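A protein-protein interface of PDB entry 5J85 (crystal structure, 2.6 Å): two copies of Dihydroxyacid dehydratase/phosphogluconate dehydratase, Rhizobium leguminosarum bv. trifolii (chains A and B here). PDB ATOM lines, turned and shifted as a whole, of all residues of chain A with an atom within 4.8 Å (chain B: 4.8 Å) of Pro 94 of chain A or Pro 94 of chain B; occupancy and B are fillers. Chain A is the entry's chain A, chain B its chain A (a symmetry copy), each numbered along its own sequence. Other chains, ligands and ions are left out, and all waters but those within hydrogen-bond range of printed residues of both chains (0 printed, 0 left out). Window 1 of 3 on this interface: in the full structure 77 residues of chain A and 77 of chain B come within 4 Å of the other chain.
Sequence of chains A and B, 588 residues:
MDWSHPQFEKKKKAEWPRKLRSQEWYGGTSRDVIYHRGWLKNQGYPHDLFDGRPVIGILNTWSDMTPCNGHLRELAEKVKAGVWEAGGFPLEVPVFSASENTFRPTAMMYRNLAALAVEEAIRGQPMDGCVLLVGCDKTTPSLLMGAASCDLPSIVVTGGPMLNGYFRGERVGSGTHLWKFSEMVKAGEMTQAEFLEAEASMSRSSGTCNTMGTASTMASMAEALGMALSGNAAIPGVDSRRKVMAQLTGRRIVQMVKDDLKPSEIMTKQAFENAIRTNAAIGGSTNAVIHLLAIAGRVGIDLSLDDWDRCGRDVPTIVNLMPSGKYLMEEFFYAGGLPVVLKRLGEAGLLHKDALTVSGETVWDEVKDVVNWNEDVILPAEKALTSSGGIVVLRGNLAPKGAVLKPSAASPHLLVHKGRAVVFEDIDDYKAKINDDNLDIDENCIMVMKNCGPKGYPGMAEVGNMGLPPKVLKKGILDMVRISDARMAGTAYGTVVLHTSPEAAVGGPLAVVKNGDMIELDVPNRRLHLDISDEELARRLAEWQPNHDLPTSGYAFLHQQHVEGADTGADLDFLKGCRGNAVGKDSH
Trp 62 of chain A touches Glu 92 of chain B. Trp 62 of chain A touches Pro 94 of chain B (O to CG, 3.6 Å). OG of Ser 63 of chain A touches O of Glu 92 of chain B (3.6 Å). Val 93 of chain B touches Ser 63 of chain A. Trp 62 of chain B touches Glu 92 of chain A (CH2 to OE2, 3.7 Å). OG of Ser 63 of chain B touches O of Glu 92 of chain A (3.6 Å). CG2 of Val 93 of chain A touches OG of Ser 63 of chain B, at 3.99 Å. Trp 62 of chain B touches Pro 94 of chain A. Pro 94 of chain B touches Pro 94 of chain A.
Asn 60 of chain A touches none of the printed residues of chain B. Of the printed residues of chain B, Glu 92 of chain A touches Trp 62 and Ser 63. Of the printed residues of chain B, Val 93 of chain A touches Ser 63. Pro 94 of chain A touches two residues of chain B. Of the printed residues of chain A, Glu 92 of chain B touches Trp 62 and Ser 63. Of the printed residues of chain A, Val 93 of chain B touches Ser 63 (3.99 Å). Pro 94 of chain B touches just these residues of chain A: Trp 62 and Pro 94. Phe 96 of chain B touches none of the printed residues of chain A. The nearest residue of chain B that does not touch Pro 94 of chain A is Ser 63 of chain B (4.04 Å).
Trp 62 of chain A touches Glu 92 of chain B, and with the chains exchanged Glu 92 of chain A touches Trp 62 of chain B. Trp 62 of chain A touches Pro 94 of chain B, and with the chains exchanged Pro 94 of chain A touches Trp 62 of chain B. Ser 63 of chain A touches Glu 92 of chain B, and with the chains exchanged Glu 92 of chain A touches Ser 63 of chain B. Pro 94 of chain B touches its own counterpart, Pro 94 of chain A. Positions printed for both chains: 60, 62, 63, 92, 93, 94, 95 and 96. Of the 9 pairs that touch across the chains among the printed residues, 9 have their exchanged pair printed and touching as well.
The backbone NH (N) of Trp 62 of chain A sits at hydrogen-bond distance from the side-chain amide oxygen (OD1) of Asn 60 of chain A (2.9 Å). The side-chain carboxylate (OE1) of Glu 92 of chain A is in hydrogen-bond range of the side-chain amide nitrogen (ND2) of Asn 60 of chain A, at 2.7 Å. N of Asn 60 of chain A is in hydrogen-bond range of O of Val 93 of chain A, at 2.9 Å. OD1 of Asn 60 of chain B is in hydrogen-bond range of N of Trp 62 of chain B (2.9 Å). The side-chain amide nitrogen of Asn 60 of chain B lies within hydrogen-bond range of the side-chain carboxylate of Glu 92 of chain B (2.7 Å). The backbone NH (N) of Asn 60 of chain B is in hydrogen-bond range of the backbone carbonyl oxygen (O) of Val 93 of chain B, 2.9 Å away.
Of the 8 printed residues of chain B, 5 touch a printed residue of chain A. Hydrophobic or aromatic side chains of chain B that line the printed part of chain A: Trp 62, Val 93 and Pro 94. Of the 8 printed residues of chain A, 5 touch a printed residue of chain B. Hydrophobic or aromatic side chains of chain A within 4 Å of the printed part of chain B: Trp 62, Val 93 and Pro 94. Among the printed residues, 9 pairs touch across the chains. Among the printed residues, no Asp or Glu carboxylate lies within 4 Å of a Lys or Arg side-chain nitrogen of the other chain.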
ATOM      1  N   ASN A  60       4.545  12.512 -11.166  1.00  0.00           N
ATOM      2  CA  ASN A  60       5.109  13.187 -10.006  1.00  0.00           C
ATOM      3  C   ASN A  60       4.275  14.417  -9.653  1.00  0.00           C
ATOM      4  O   ASN A  60       4.157  15.339 -10.469  1.00  0.00           O
ATOM      5  CB  ASN A  60       6.560  13.569 -10.279  1.00  0.00           C
ATOM      6  CG  ASN A  60       7.277  13.972  -9.033  1.00  0.00           C
ATOM      7  OD1 ASN A  60       6.651  14.127  -7.982  1.00  0.00           O
ATOM      8  ND2 ASN A  60       8.595  14.141  -9.122  1.00  0.00           N
ATOM      9  N   TRP A  62       5.137  16.521  -7.361  1.00  0.00           N
ATOM     10  CA  TRP A  62       5.991  17.522  -6.748  1.00  0.00           C
ATOM     11  C   TRP A  62       5.677  18.907  -7.305  1.00  0.00           C
ATOM     12  O   TRP A  62       5.359  19.073  -8.487  1.00  0.00           O
ATOM     13  CB  TRP A  62       7.463  17.214  -6.986  1.00  0.00           C
ATOM     14  CG  TRP A  62       8.339  18.372  -6.575  1.00  0.00           C
ATOM     15  CD1 TRP A  62       8.897  18.583  -5.346  1.00  0.00           C
ATOM     16  CD2 TRP A  62       8.722  19.490  -7.383  1.00  0.00           C
ATOM     17  NE1 TRP A  62       9.618  19.751  -5.344  1.00  0.00           N
ATOM     18  CE2 TRP A  62       9.521  20.333  -6.579  1.00  0.00           C
ATOM     19  CE3 TRP A  62       8.473  19.858  -8.712  1.00  0.00           C
ATOM     20  CZ2 TRP A  62      10.072  21.524  -7.059  1.00  0.00           C
ATOM     21  CZ3 TRP A  62       9.025  21.044  -9.191  1.00  0.00           C
ATOM     22  CH2 TRP A  62       9.816  21.862  -8.361  1.00  0.00           C
ATOM     23  N   SER A  63       5.786  19.909  -6.434  1.00  0.00           N
ATOM     24  CA  SER A  63       5.638  21.310  -6.800  1.00  0.00           C
ATOM     25  C   SER A  63       6.229  22.156  -5.685  1.00  0.00           C
ATOM     26  O   SER A  63       6.178  21.776  -4.517  1.00  0.00           O
ATOM     27  CB  SER A  63       4.174  21.678  -7.026  1.00  0.00           C
ATOM     28  OG  SER A  63       4.040  23.070  -7.160  1.00  0.00           O
ATOM     29  N   GLU A  92       9.923  10.554 -16.236  1.00  0.00           N
ATOM     30  CA  GLU A  92       9.181  11.330 -15.247  1.00  0.00           C
ATOM     31  C   GLU A  92       8.169  12.248 -15.928  1.00  0.00           C
ATOM     32  O   GLU A  92       8.481  12.923 -16.910  1.00  0.00           O
ATOM     33  CB  GLU A  92      10.129  12.147 -14.373  1.00  0.00           C
ATOM     34  CG  GLU A  92       9.400  12.877 -13.253  1.00  0.00           C
ATOM     35  CD  GLU A  92      10.330  13.683 -12.355  1.00  0.00           C
ATOM     36  OE1 GLU A  92       9.813  14.463 -11.522  1.00  0.00           O
ATOM     37  OE2 GLU A  92      11.570  13.535 -12.477  1.00  0.00           O
ATOM     38  N   VAL A  93       6.950  12.261 -15.412  1.00  0.00           N
ATOM     39  CA  VAL A  93       5.875  13.071 -15.979  1.00  0.00           C
ATOM     40  C   VAL A  93       5.222  13.856 -14.847  1.00  0.00           C
ATOM     41  O   VAL A  93       4.519  13.265 -14.015  1.00  0.00           O
ATOM     42  CB  VAL A  93       4.836  12.197 -16.701  1.00  0.00           C
ATOM     43  CG1 VAL A  93       3.638  13.026 -17.142  1.00  0.00           C
ATOM     44  CG2 VAL A  93       5.465  11.488 -17.874  1.00  0.00           C
ATOM     45  N   PRO A  94       5.428  15.167 -14.761  1.00  0.00           N
ATOM     46  CA  PRO A  94       4.714  15.953 -13.747  1.00  0.00           C
ATOM     47  C   PRO A  94       3.220  15.972 -14.019  1.00  0.00           C
ATOM     48  O   PRO A  94       2.775  15.952 -15.170  1.00  0.00           O
ATOM     49  CB  PRO A  94       5.326  17.350 -13.888  1.00  0.00           C
ATOM     50  CG  PRO A  94       6.707  17.085 -14.499  1.00  0.00           C
ATOM     51  CD  PRO A  94       6.448  15.961 -15.468  1.00  0.00           C
ATOM     52  N   VAL A  95       2.433  15.972 -12.938  1.00  0.00           N
ATOM     53  CA  VAL A  95       0.981  16.066 -13.048  1.00  0.00           C
ATOM     54  C   VAL A  95       0.448  17.108 -12.068  1.00  0.00           C
ATOM     55  O   VAL A  95       1.120  17.507 -11.111  1.00  0.00           O
ATOM     56  CB  VAL A  95       0.279  14.708 -12.817  1.00  0.00           C
ATOM     57  CG1 VAL A  95       0.605  13.747 -13.943  1.00  0.00           C
ATOM     58  CG2 VAL A  95       0.679  14.118 -11.487  1.00  0.00           C
ATOM     59  N   PHE A  96      -0.796  17.530 -12.330  1.00  0.00           N
ATOM     60  CA  PHE A  96      -1.486  18.547 -11.538  1.00  0.00           C
ATOM     61  C   PHE A  96      -1.486  18.199 -10.056  1.00  0.00           C
ATOM     62  O   PHE A  96      -1.937  17.119  -9.660  1.00  0.00           O
ATOM     63  CB  PHE A  96      -2.922  18.687 -12.040  1.00  0.00           C
ATOM     64  CG  PHE A  96      -3.629  19.914 -11.539  1.00  0.00           C
ATOM     65  CD1 PHE A  96      -4.225  19.931 -10.285  1.00  0.00           C
ATOM     66  CD2 PHE A  96      -3.706  21.052 -12.324  1.00  0.00           C
ATOM     67  CE1 PHE A  96      -4.875  21.054  -9.832  1.00  0.00           C
ATOM     68  CE2 PHE A  96      -4.359  22.182 -11.869  1.00  0.00           C
ATOM     69  CZ  PHE A  96      -4.941  22.179 -10.622  1.00  0.00           C
ATOM     70  N   ASN B  60       6.241  25.465 -15.436  1.00  0.00           N
ATOM     71  CA  ASN B  60       7.235  24.719 -16.194  1.00  0.00           C
ATOM     72  C   ASN B  60       6.573  23.558 -16.933  1.00  0.00           C
ATOM     73  O   ASN B  60       5.997  22.668 -16.296  1.00  0.00           O
ATOM     74  CB  ASN B  60       8.335  24.221 -15.262  1.00  0.00           C
ATOM     75  CG  ASN B  60       9.526  23.730 -16.016  1.00  0.00           C
ATOM     76  OD1 ASN B  60       9.476  23.606 -17.241  1.00  0.00           O
ATOM     77  ND2 ASN B  60      10.618  23.451 -15.304  1.00  0.00           N
ATOM     78  N   TRP B  62       8.251  21.337 -18.569  1.00  0.00           N
ATOM     79  CA  TRP B  62       9.206  20.253 -18.715  1.00  0.00           C
ATOM     80  C   TRP B  62       8.544  18.913 -18.410  1.00  0.00           C
ATOM     81  O   TRP B  62       7.682  18.802 -17.532  1.00  0.00           O
ATOM     82  CB  TRP B  62      10.399  20.440 -17.789  1.00  0.00           C
ATOM     83  CG  TRP B  62      11.262  19.202 -17.751  1.00  0.00           C
ATOM     84  CD1 TRP B  62      12.324  18.916 -18.562  1.00  0.00           C
ATOM     85  CD2 TRP B  62      11.110  18.073 -16.884  1.00  0.00           C
ATOM     86  NE1 TRP B  62      12.853  17.691 -18.242  1.00  0.00           N
ATOM     87  CE2 TRP B  62      12.122  17.147 -17.220  1.00  0.00           C
ATOM     88  CE3 TRP B  62      10.219  17.758 -15.849  1.00  0.00           C
ATOM     89  CZ2 TRP B  62      12.268  15.924 -16.561  1.00  0.00           C
ATOM     90  CZ3 TRP B  62      10.367  16.540 -15.190  1.00  0.00           C
ATOM     91  CH2 TRP B  62      11.387  15.638 -15.552  1.00  0.00           C
ATOM     92  N   SER B  63       8.974  17.887 -19.142  1.00  0.00           N
ATOM     93  CA  SER B  63       8.548  16.512 -18.925  1.00  0.00           C
ATOM     94  C   SER B  63       9.529  15.594 -19.634  1.00  0.00           C
ATOM     95  O   SER B  63      10.081  15.951 -20.671  1.00  0.00           O
ATOM     96  CB  SER B  63       7.132  16.275 -19.442  1.00  0.00           C
ATOM     97  OG  SER B  63       6.831  14.904 -19.420  1.00  0.00           O
ATOM     98  N   GLU B  92       8.646  27.067  -8.357  1.00  0.00           N
ATOM     99  CA  GLU B  92       8.410  26.335  -9.599  1.00  0.00           C
ATOM    100  C   GLU B  92       7.121  25.523  -9.511  1.00  0.00           C
ATOM    101  O   GLU B  92       6.861  24.846  -8.516  1.00  0.00           O
ATOM    102  CB  GLU B  92       9.589  25.421  -9.923  1.00  0.00           C
ATOM    103  CG  GLU B  92       9.432  24.732 -11.272  1.00  0.00           C
ATOM    104  CD  GLU B  92      10.607  23.829 -11.626  1.00  0.00           C
ATOM    105  OE1 GLU B  92      10.492  23.079 -12.623  1.00  0.00           O
ATOM    106  OE2 GLU B  92      11.642  23.873 -10.917  1.00  0.00           O
ATOM    107  N   VAL B  93       6.307  25.603 -10.552  1.00  0.00           N
ATOM    108  CA  VAL B  93       5.027  24.901 -10.593  1.00  0.00           C
ATOM    109  C   VAL B  93       4.937  24.150 -11.916  1.00  0.00           C
ATOM    110  O   VAL B  93       4.777  24.781 -12.971  1.00  0.00           O
ATOM    111  CB  VAL B  93       3.848  25.877 -10.444  1.00  0.00           C
ATOM    112  CG1 VAL B  93       2.520  25.164 -10.655  1.00  0.00           C
ATOM    113  CG2 VAL B  93       3.890  26.555  -9.097  1.00  0.00           C
ATOM    114  N   PRO B  94       5.046  22.825 -11.921  1.00  0.00           N
ATOM    115  CA  PRO B  94       4.846  22.081 -13.172  1.00  0.00           C
ATOM    116  C   PRO B  94       3.411  22.196 -13.656  1.00  0.00           C
ATOM    117  O   PRO B  94       2.470  22.279 -12.862  1.00  0.00           O
ATOM    118  CB  PRO B  94       5.192  20.640 -12.783  1.00  0.00           C
ATOM    119  CG  PRO B  94       6.122  20.800 -11.576  1.00  0.00           C
ATOM    120  CD  PRO B  94       5.525  21.962 -10.827  1.00  0.00           C
ATOM    121  N   VAL B  95       3.248  22.240 -14.981  1.00  0.00           N
ATOM    122  CA  VAL B  95       1.922  22.273 -15.589  1.00  0.00           C
ATOM    123  C   VAL B  95       1.841  21.259 -16.727  1.00  0.00           C
ATOM    124  O   VAL B  95       2.855  20.783 -17.249  1.00  0.00           O
ATOM    125  CB  VAL B  95       1.538  23.681 -16.101  1.00  0.00           C
ATOM    126  CG1 VAL B  95       1.361  24.635 -14.936  1.00  0.00           C
ATOM    127  CG2 VAL B  95       2.580  24.205 -17.058  1.00  0.00           C
ATOM    128  N   PHE B  96       0.595  20.951 -17.108  1.00  0.00           N
ATOM    129  CA  PHE B  96       0.288  19.980 -18.157  1.00  0.00           C
ATOM    130  C   PHE B  96       1.034  20.294 -19.447  1.00  0.00           C
ATOM    131  O   PHE B  96       0.925  21.400 -19.988  1.00  0.00           O
ATOM    132  CB  PHE B  96      -1.217  19.975 -18.414  1.00  0.00           C
ATOM    133  CG  PHE B  96      -1.696  18.803 -19.222  1.00  0.00           C
ATOM    134  CD1 PHE B  96      -1.612  18.808 -20.608  1.00  0.00           C
ATOM    135  CD2 PHE B  96      -2.240  17.693 -18.598  1.00  0.00           C
ATOM    136  CE1 PHE B  96      -2.056  17.736 -21.343  1.00  0.00           C
ATOM    137  CE2 PHE B  96      -2.686  16.613 -19.336  1.00  0.00           C
ATOM    138  CZ  PHE B  96      -2.591  16.638 -20.708  1.00  0.00           C
